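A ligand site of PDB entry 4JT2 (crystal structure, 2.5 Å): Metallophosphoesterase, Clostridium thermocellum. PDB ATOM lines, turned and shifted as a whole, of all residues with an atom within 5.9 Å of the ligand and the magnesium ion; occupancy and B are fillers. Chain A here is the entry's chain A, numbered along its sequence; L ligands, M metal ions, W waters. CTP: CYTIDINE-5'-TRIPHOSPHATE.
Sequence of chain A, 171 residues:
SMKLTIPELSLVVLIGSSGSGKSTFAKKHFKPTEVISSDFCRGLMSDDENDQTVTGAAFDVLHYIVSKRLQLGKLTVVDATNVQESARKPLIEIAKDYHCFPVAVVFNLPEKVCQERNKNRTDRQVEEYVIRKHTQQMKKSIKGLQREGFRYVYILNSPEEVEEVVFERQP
The backbone NH of Ser 23 is in hydrogen-bond range of an oxygen (O1A) of the ligand, at 3.1 Å.
An oxygen (O1B) of the ligand is in hydrogen-bond range of the backbone NH of Gly 21, at 3.1 Å.
N of Thr 24 lies within hydrogen-bond range of O1A of the ligand, at 2.8 Å.
O1B of the ligand lies within hydrogen-bond range of N of Lys 22.
O2G of the ligand lies within salt-bridge range of NH1 of Arg 121.
An oxygen (O3B) of the ligand lies within hydrogen-bond range of the backbone NH of Gly 19 (3.2 Å).
O2G of the ligand lies within salt-bridge range of NH1 of Arg 124, 2.9 Å away.
OG1 of Thr 24 is in hydrogen-bond range of O1A of the ligand (2.9 Å).
NZ of Lys 22 is in salt-bridge range of O1B of the ligand, 2.7 Å away.
OG of Ser 18 is in hydrogen-bond range of O2G of the ligand.
O of Ser 20 lies within hydrogen-bond range of NH1 of Arg 117 (3.0 Å).
The guanidinium group (NH2) of Arg 121 lies within salt-bridge range of the side-chain carboxylate (OD2) of Asp 123 (2.7 Å).
N of Ser 18 sits at hydrogen-bond distance from ND1 of His 134 (3.2 Å).
The side-chain carboxylate of Asp 79 lies close to the side-chain hydroxyl of Ser 23, 3.4 Å away.
The guanidinium group (NE) of Arg 121 sits at hydrogen-bond distance from the backbone carbonyl oxygen (O) of Arg 124 (3.0 Å).
O of Ser 17 sits at hydrogen-bond distance from OG of Ser 20, at 2.7 Å.
The side-chain amino group of Lys 22 lies within hydrogen-bond range of the backbone carbonyl oxygen of Gly 16 (3.0 Å).
O of Ser 17 is in hydrogen-bond range of NZ of Lys 22, 2.9 Å away.
Merely in contact with the ligand: Arg 117, Ser 17 and Ser 20.
Within 4 Å of the ligand: Ser 17, Ser 18, Gly 19, Ser 20, Gly 21, Lys 22, Ser 23, Thr 24, Arg 117, Arg 121 and Arg 124.
Asp 79 touches the magnesium ion (OD2 to MG, 3.9 Å).
Arg 124 touches the magnesium ion (NH2 to MG, 3.5 Å).
Of the 24 residues printed, 3 come within 4 Å of the magnesium ion.
The nearest printed residue that does not touch the magnesium ion is Arg 121 (4.7 Å).
The magnesium ion is bound by O3G of the ligand, water W6, O2B of the ligand, water W9, water W7 and OG of Ser 23.
Water W6 lies within hydrogen-bond range of an oxygen (O2A) of the ligand (2.7 Å), the guanidinium group (NH2) of Arg 121 (3.2 Å) and the guanidinium group (NH2) of Arg 124 (3.2 Å).
Water W5 lies within hydrogen-bond range of the side-chain carboxylate (OD2) of Asp 123 (2.6 Å), an oxygen (O2A) of the ligand (2.7 Å) and the guanidinium group (NH2) of Arg 121 (3.3 Å).
Water W8 lies within hydrogen-bond range of the backbone carbonyl oxygen (O) of Arg 117, an oxygen (O3') of the ligand and the backbone NH (N) of Arg 121.
Water W3 lies within hydrogen-bond range of OG1 of Thr 122, OD1 of Asp 123 and O3' of the ligand.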
ATOM      1  N   GLY A  16      -7.741 -22.213  34.133  1.00  0.00           N
ATOM      2  CA  GLY A  16      -8.143 -20.827  34.241  1.00  0.00           C
ATOM      3  C   GLY A  16      -9.637 -20.655  34.477  1.00  0.00           C
ATOM      4  O   GLY A  16     -10.460 -21.497  34.099  1.00  0.00           O
ATOM      5  N   SER A  17      -9.974 -19.529  35.112  1.00  0.00           N
ATOM      6  CA  SER A  17     -11.350 -19.136  35.339  1.00  0.00           C
ATOM      7  C   SER A  17     -12.127 -19.013  34.032  1.00  0.00           C
ATOM      8  O   SER A  17     -11.536 -18.926  32.966  1.00  0.00           O
ATOM      9  CB  SER A  17     -11.376 -17.792  36.061  1.00  0.00           C
ATOM     10  OG  SER A  17     -12.695 -17.313  36.185  1.00  0.00           O
ATOM     11  N   SER A  18     -13.438 -19.016  34.135  1.00  0.00           N
ATOM     12  CA  SER A  18     -14.251 -18.614  33.004  1.00  0.00           C
ATOM     13  C   SER A  18     -13.872 -17.180  32.655  1.00  0.00           C
ATOM     14  O   SER A  18     -13.674 -16.362  33.552  1.00  0.00           O
ATOM     15  CB  SER A  18     -15.741 -18.678  33.350  1.00  0.00           C
ATOM     16  OG  SER A  18     -16.550 -18.372  32.233  1.00  0.00           O
ATOM     17  N   GLY A  19     -13.735 -16.889  31.368  1.00  0.00           N
ATOM     18  CA  GLY A  19     -13.359 -15.546  30.929  1.00  0.00           C
ATOM     19  C   GLY A  19     -11.858 -15.322  30.839  1.00  0.00           C
ATOM     20  O   GLY A  19     -11.416 -14.275  30.363  1.00  0.00           O
ATOM     21  N   SER A  20     -11.071 -16.302  31.284  1.00  0.00           N
ATOM     22  CA  SER A  20      -9.625 -16.139  31.277  1.00  0.00           C
ATOM     23  C   SER A  20      -9.037 -16.298  29.866  1.00  0.00           C
ATOM     24  O   SER A  20      -7.876 -15.911  29.630  1.00  0.00           O
ATOM     25  CB  SER A  20      -8.950 -17.095  32.267  1.00  0.00           C
ATOM     26  OG  SER A  20      -9.084 -18.450  31.876  1.00  0.00           O
ATOM     27  N   GLY A  21      -9.828 -16.843  28.945  1.00  0.00           N
ATOM     28  CA  GLY A  21      -9.462 -16.868  27.536  1.00  0.00           C
ATOM     29  C   GLY A  21      -8.901 -18.180  27.007  1.00  0.00           C
ATOM     30  O   GLY A  21      -8.202 -18.185  25.987  1.00  0.00           O
ATOM     31  N   LYS A  22      -9.229 -19.283  27.674  1.00  0.00           N
ATOM     32  CA  LYS A  22      -8.721 -20.609  27.300  1.00  0.00           C
ATOM     33  C   LYS A  22      -9.063 -21.051  25.862  1.00  0.00           C
ATOM     34  O   LYS A  22      -8.171 -21.430  25.086  1.00  0.00           O
ATOM     35  CB  LYS A  22      -9.224 -21.663  28.293  1.00  0.00           C
ATOM     36  CG  LYS A  22      -8.868 -21.361  29.743  1.00  0.00           C
ATOM     37  CD  LYS A  22      -9.402 -22.432  30.699  1.00  0.00           C
ATOM     38  CE  LYS A  22     -10.926 -22.487  30.697  1.00  0.00           C
ATOM     39  NZ  LYS A  22     -11.515 -21.262  31.282  1.00  0.00           N
ATOM     40  N   SER A  23     -10.350 -20.983  25.513  1.00  0.00           N
ATOM     41  CA  SER A  23     -10.785 -21.405  24.182  1.00  0.00           C
ATOM     42  C   SER A  23     -10.208 -20.553  23.053  1.00  0.00           C
ATOM     43  O   SER A  23      -9.860 -21.055  21.969  1.00  0.00           O
ATOM     44  CB  SER A  23     -12.321 -21.453  24.107  1.00  0.00           C
ATOM     45  OG  SER A  23     -12.876 -22.304  25.098  1.00  0.00           O
ATOM     46  N   THR A  24     -10.139 -19.244  23.296  1.00  0.00           N
ATOM     47  CA  THR A  24      -9.462 -18.323  22.385  1.00  0.00           C
ATOM     48  C   THR A  24      -8.023 -18.782  22.147  1.00  0.00           C
ATOM     49  O   THR A  24      -7.574 -18.903  21.012  1.00  0.00           O
ATOM     50  CB  THR A  24      -9.452 -16.901  22.957  1.00  0.00           C
ATOM     51  OG1 THR A  24     -10.797 -16.486  23.207  1.00  0.00           O
ATOM     52  CG2 THR A  24      -8.760 -15.943  21.993  1.00  0.00           C
ATOM     53  N   PHE A  25      -7.326 -19.076  23.247  1.00  0.00           N
ATOM     54  CA  PHE A  25      -5.940 -19.551  23.232  1.00  0.00           C
ATOM     55  C   PHE A  25      -5.830 -20.860  22.446  1.00  0.00           C
ATOM     56  O   PHE A  25      -5.008 -20.992  21.534  1.00  0.00           O
ATOM     57  CB  PHE A  25      -5.479 -19.710  24.684  1.00  0.00           C
ATOM     58  CG  PHE A  25      -4.029 -20.067  24.846  1.00  0.00           C
ATOM     59  CD1 PHE A  25      -3.642 -21.392  25.000  1.00  0.00           C
ATOM     60  CD2 PHE A  25      -3.065 -19.076  24.926  1.00  0.00           C
ATOM     61  CE1 PHE A  25      -2.315 -21.724  25.181  1.00  0.00           C
ATOM     62  CE2 PHE A  25      -1.731 -19.396  25.104  1.00  0.00           C
ATOM     63  CZ  PHE A  25      -1.351 -20.722  25.234  1.00  0.00           C
ATOM     64  N   ASP A  79      -9.678 -28.243  27.036  1.00  0.00           N
ATOM     65  CA  ASP A  79     -10.194 -26.904  27.224  1.00  0.00           C
ATOM     66  C   ASP A  79     -11.316 -26.943  28.258  1.00  0.00           C
ATOM     67  O   ASP A  79     -12.492 -27.109  27.897  1.00  0.00           O
ATOM     68  CB  ASP A  79     -10.706 -26.332  25.894  1.00  0.00           C
ATOM     69  CG  ASP A  79     -11.251 -24.926  26.025  1.00  0.00           C
ATOM     70  OD1 ASP A  79     -11.006 -24.277  27.067  1.00  0.00           O
ATOM     71  OD2 ASP A  79     -11.935 -24.461  25.079  1.00  0.00           O
ATOM     72  N   ALA A  80     -10.961 -26.800  29.521  1.00  0.00           N
ATOM     73  CA  ALA A  80     -11.951 -26.727  30.601  1.00  0.00           C
ATOM     74  C   ALA A  80     -11.362 -25.841  31.677  1.00  0.00           C
ATOM     75  O   ALA A  80     -10.208 -25.468  31.588  1.00  0.00           O
ATOM     76  CB  ALA A  80     -12.258 -28.123  31.148  1.00  0.00           C
ATOM     77  N   THR A  81     -12.146 -25.503  32.703  1.00  0.00           N
ATOM     78  CA  THR A  81     -11.657 -24.629  33.752  1.00  0.00           C
ATOM     79  C   THR A  81     -10.464 -25.253  34.486  1.00  0.00           C
ATOM     80  O   THR A  81      -9.417 -24.613  34.621  1.00  0.00           O
ATOM     81  CB  THR A  81     -12.748 -24.237  34.771  1.00  0.00           C
ATOM     82  OG1 THR A  81     -13.131 -25.381  35.535  1.00  0.00           O
ATOM     83  CG2 THR A  81     -13.956 -23.664  34.062  1.00  0.00           C
ATOM     84  N   ARG A 117     -14.198  -9.438  30.609  1.00  0.00           N
ATOM     85  CA  ARG A 117     -14.377 -10.157  29.347  1.00  0.00           C
ATOM     86  C   ARG A 117     -15.711 -10.870  29.337  1.00  0.00           C
ATOM     87  O   ARG A 117     -16.409 -10.920  28.319  1.00  0.00           O
ATOM     88  CB  ARG A 117     -13.251 -11.162  29.132  1.00  0.00           C
ATOM     89  CG  ARG A 117     -11.875 -10.540  28.923  1.00  0.00           C
ATOM     90  CD  ARG A 117     -10.799 -11.611  28.849  1.00  0.00           C
ATOM     91  NE  ARG A 117      -9.505 -11.098  28.419  1.00  0.00           N
ATOM     92  CZ  ARG A 117      -8.369 -11.816  28.413  1.00  0.00           C
ATOM     93  NH1 ARG A 117      -8.374 -13.069  28.827  1.00  0.00           N
ATOM     94  NH2 ARG A 117      -7.241 -11.257  28.003  1.00  0.00           N
ATOM     95  N   ASN A 118     -16.058 -11.421  30.496  1.00  0.00           N
ATOM     96  CA  ASN A 118     -17.332 -12.091  30.678  1.00  0.00           C
ATOM     97  C   ASN A 118     -18.526 -11.220  30.320  1.00  0.00           C
ATOM     98  O   ASN A 118     -19.450 -11.680  29.647  1.00  0.00           O
ATOM     99  CB  ASN A 118     -17.461 -12.546  32.127  1.00  0.00           C
ATOM    100  CG  ASN A 118     -18.744 -13.301  32.382  1.00  0.00           C
ATOM    101  OD1 ASN A 118     -19.057 -14.274  31.704  1.00  0.00           O
ATOM    102  ND2 ASN A 118     -19.495 -12.845  33.365  1.00  0.00           N
ATOM    103  N   ASN A 120     -18.758  -8.961  28.270  1.00  0.00           N
ATOM    104  CA  ASN A 120     -18.770  -8.606  26.857  1.00  0.00           C
ATOM    105  C   ASN A 120     -18.874  -9.812  25.909  1.00  0.00           C
ATOM    106  O   ASN A 120     -18.919  -9.639  24.696  1.00  0.00           O
ATOM    107  CB  ASN A 120     -17.549  -7.743  26.509  1.00  0.00           C
ATOM    108  CG  ASN A 120     -17.598  -6.374  27.181  1.00  0.00           C
ATOM    109  OD1 ASN A 120     -18.608  -5.663  27.108  1.00  0.00           O
ATOM    110  ND2 ASN A 120     -16.492  -5.996  27.820  1.00  0.00           N
ATOM    111  N   ARG A 121     -18.913 -11.016  26.472  1.00  0.00           N
ATOM    112  CA  ARG A 121     -19.079 -12.244  25.690  1.00  0.00           C
ATOM    113  C   ARG A 121     -20.402 -12.287  24.914  1.00  0.00           C
ATOM    114  O   ARG A 121     -21.456 -11.884  25.418  1.00  0.00           O
ATOM    115  CB  ARG A 121     -19.004 -13.486  26.582  1.00  0.00           C
ATOM    116  CG  ARG A 121     -17.705 -13.632  27.319  1.00  0.00           C
ATOM    117  CD  ARG A 121     -17.677 -14.937  28.063  1.00  0.00           C
ATOM    118  NE  ARG A 121     -17.735 -16.090  27.166  1.00  0.00           N
ATOM    119  CZ  ARG A 121     -17.327 -17.305  27.509  1.00  0.00           C
ATOM    120  NH1 ARG A 121     -16.845 -17.525  28.723  1.00  0.00           N
ATOM    121  NH2 ARG A 121     -17.395 -18.313  26.633  1.00  0.00           N
ATOM    122  N   THR A 122     -20.346 -12.825  23.695  1.00  0.00           N
ATOM    123  CA  THR A 122     -21.531 -12.914  22.869  1.00  0.00           C
ATOM    124  C   THR A 122     -22.031 -14.335  22.796  1.00  0.00           C
ATOM    125  O   THR A 122     -23.119 -14.605  22.301  1.00  0.00           O
ATOM    126  CB  THR A 122     -21.266 -12.427  21.440  1.00  0.00           C
ATOM    127  OG1 THR A 122     -20.169 -13.175  20.887  1.00  0.00           O
ATOM    128  CG2 THR A 122     -20.913 -10.940  21.441  1.00  0.00           C
ATOM    129  N   ASP A 123     -21.234 -15.279  23.287  1.00  0.00           N
ATOM    130  CA  ASP A 123     -21.650 -16.674  23.232  1.00  0.00           C
ATOM    131  C   ASP A 123     -22.461 -17.109  24.455  1.00  0.00           C
ATOM    132  O   ASP A 123     -23.579 -17.561  24.329  1.00  0.00           O
ATOM    133  CB  ASP A 123     -20.450 -17.614  23.005  1.00  0.00           C
ATOM    134  CG  ASP A 123     -19.288 -17.300  23.930  1.00  0.00           C
ATOM    135  OD1 ASP A 123     -19.212 -16.175  24.464  1.00  0.00           O
ATOM    136  OD2 ASP A 123     -18.424 -18.199  24.103  1.00  0.00           O
ATOM    137  N   ARG A 124     -21.881 -16.945  25.627  1.00  0.00           N
ATOM    138  CA  ARG A 124     -22.564 -17.254  26.878  1.00  0.00           C
ATOM    139  C   ARG A 124     -21.856 -16.518  28.014  1.00  0.00           C
ATOM    140  O   ARG A 124     -20.664 -16.201  27.902  1.00  0.00           O
ATOM    141  CB  ARG A 124     -22.541 -18.751  27.146  1.00  0.00           C
ATOM    142  CG  ARG A 124     -21.137 -19.321  27.138  1.00  0.00           C
ATOM    143  CD  ARG A 124     -21.106 -20.835  27.269  1.00  0.00           C
ATOM    144  NE  ARG A 124     -19.756 -21.335  27.007  1.00  0.00           N
ATOM    145  CZ  ARG A 124     -18.768 -21.376  27.896  1.00  0.00           C
ATOM    146  NH1 ARG A 124     -18.980 -20.978  29.150  1.00  0.00           N
ATOM    147  NH2 ARG A 124     -17.571 -21.836  27.536  1.00  0.00           N
ATOM    148  N   VAL A 126     -21.440 -16.146  32.539  1.00  0.00           N
ATOM    149  CA  VAL A 126     -21.653 -16.738  33.856  1.00  0.00           C
ATOM    150  C   VAL A 126     -21.875 -15.656  34.901  1.00  0.00           C
ATOM    151  O   VAL A 126     -21.607 -14.473  34.664  1.00  0.00           O
ATOM    152  CB  VAL A 126     -20.467 -17.627  34.307  1.00  0.00           C
ATOM    153  CG1 VAL A 126     -20.148 -18.672  33.247  1.00  0.00           C
ATOM    154  CG2 VAL A 126     -19.240 -16.781  34.624  1.00  0.00           C
ATOM    155  N   HIS A 134     -13.675 -19.352  40.802  1.00  0.00           N
ATOM    156  CA  HIS A 134     -12.681 -19.927  39.908  1.00  0.00           C
ATOM    157  C   HIS A 134     -11.293 -19.325  40.132  1.00  0.00           C
ATOM    158  O   HIS A 134     -10.298 -20.057  40.220  1.00  0.00           O
ATOM    159  CB  HIS A 134     -13.087 -19.690  38.456  1.00  0.00           C
ATOM    160  CG  HIS A 134     -14.162 -20.591  37.963  1.00  0.00           C
ATOM    161  ND1 HIS A 134     -14.642 -20.557  36.673  1.00  0.00           N
ATOM    162  CD2 HIS A 134     -14.858 -21.567  38.599  1.00  0.00           C
ATOM    163  CE1 HIS A 134     -15.585 -21.468  36.527  1.00  0.00           C
ATOM    164  NE2 HIS A 134     -15.733 -22.095  37.677  1.00  0.00           N
ATOM    165  N   VAL A 162       0.364 -13.997  27.844  1.00  0.00           N
ATOM    166  CA  VAL A 162      -0.492 -14.953  27.152  1.00  0.00           C
ATOM    167  C   VAL A 162      -0.397 -14.710  25.648  1.00  0.00           C
ATOM    168  O   VAL A 162      -0.291 -15.642  24.855  1.00  0.00           O
ATOM    169  CB  VAL A 162      -1.951 -14.787  27.592  1.00  0.00           C
ATOM    170  CG1 VAL A 162      -2.896 -15.593  26.672  1.00  0.00           C
ATOM    171  CG2 VAL A 162      -2.111 -15.198  29.059  1.00  0.00           C
ATOM    172  N   GLU A 163      -0.428 -13.440  25.272  1.00  0.00           N
ATOM    173  CA  GLU A 163      -0.338 -13.019  23.877  1.00  0.00           C
ATOM    174  C   GLU A 163       0.964 -13.476  23.206  1.00  0.00           C
ATOM    175  O   GLU A 163       0.958 -13.921  22.055  1.00  0.00           O
ATOM    176  CB  GLU A 163      -0.441 -11.495  23.819  1.00  0.00           C
ATOM    177  CG  GLU A 163      -1.680 -10.984  23.123  1.00  0.00           C
ATOM    178  CD  GLU A 163      -1.507 -10.956  21.622  1.00  0.00           C
ATOM    179  OE1 GLU A 163      -2.502 -10.682  20.913  1.00  0.00           O
ATOM    180  OE2 GLU A 163      -0.372 -11.200  21.152  1.00  0.00           O
HETATM  181  N1  CTP L   1     -10.985 -12.627  25.023  1.00  0.00           N
HETATM  182  C2  CTP L   1     -10.343 -11.402  24.802  1.00  0.00           C
HETATM  183  N3  CTP L   1      -8.998 -11.335  24.664  1.00  0.00           N
HETATM  184  C4  CTP L   1      -8.266 -12.475  24.716  1.00  0.00           C
HETATM  185  C5  CTP L   1      -8.884 -13.699  24.923  1.00  0.00           C
HETATM  186  C6  CTP L   1     -10.268 -13.758  25.079  1.00  0.00           C
HETATM  187  O2  CTP L   1     -11.034 -10.362  24.755  1.00  0.00           O
HETATM  188  N4  CTP L   1      -6.928 -12.415  24.568  1.00  0.00           N
HETATM  189  C1' CTP L   1     -12.438 -12.647  25.166  1.00  0.00           C
HETATM  190  C2' CTP L   1     -13.043 -13.596  24.140  1.00  0.00           C
HETATM  191  O2' CTP L   1     -13.334 -12.910  22.916  1.00  0.00           O
HETATM  192  C3' CTP L   1     -14.324 -14.025  24.810  1.00  0.00           C
HETATM  193  C4' CTP L   1     -14.034 -13.923  26.301  1.00  0.00           C
HETATM  194  O4' CTP L   1     -12.837 -13.147  26.445  1.00  0.00           O
HETATM  195  O3' CTP L   1     -15.311 -13.048  24.524  1.00  0.00           O
HETATM  196  C5' CTP L   1     -13.864 -15.322  26.891  1.00  0.00           C
HETATM  197  O5' CTP L   1     -12.797 -16.006  26.227  1.00  0.00           O
HETATM  198  PA  CTP L   1     -12.854 -17.598  26.159  1.00  0.00           P
HETATM  199  O1A CTP L   1     -11.671 -18.137  25.424  1.00  0.00           O
HETATM  200  O2A CTP L   1     -14.239 -17.975  25.675  1.00  0.00           O
HETATM  201  O3A CTP L   1     -12.746 -17.860  27.747  1.00  0.00           O
HETATM  202  PB  CTP L   1     -12.745 -19.315  28.438  1.00  0.00           P
HETATM  203  O1B CTP L   1     -11.634 -19.314  29.472  1.00  0.00           O
HETATM  204  O2B CTP L   1     -12.782 -20.370  27.367  1.00  0.00           O
HETATM  205  O3B CTP L   1     -14.133 -19.290  29.262  1.00  0.00           O
HETATM  206  PG  CTP L   1     -15.007 -20.605  29.654  1.00  0.00           P
HETATM  207  O1G CTP L   1     -14.406 -21.180  30.914  1.00  0.00           O
HETATM  208  O2G CTP L   1     -16.328 -19.966  29.919  1.00  0.00           O
HETATM  209  O3G CTP L   1     -14.935 -21.502  28.449  1.00  0.00           O
HETATM  210 MG    MG M   1     -14.112 -21.713  26.810  1.00  0.00          MG
HETATM  211  O   HOH W   1      -3.951 -13.251  23.560  1.00  0.00           O
HETATM  212  O   HOH W   2     -14.449 -24.147  30.210  1.00  0.00           O
HETATM  213  O   HOH W   3     -17.750 -14.337  22.390  1.00  0.00           O
HETATM  214  O   HOH W   4      -6.613 -16.142  25.469  1.00  0.00           O
HETATM  215  O   HOH W   5     -16.033 -17.324  23.748  1.00  0.00           O
HETATM  216  O   HOH W   6     -15.134 -20.474  25.882  1.00  0.00           O
HETATM  217  O   HOH W   7     -15.322 -23.299  26.214  1.00  0.00           O
HETATM  218  O   HOH W   8     -15.678 -10.638  25.858  1.00  0.00           O
HETATM  219  O   HOH W   9     -13.330 -23.300  27.688  1.00  0.00           O
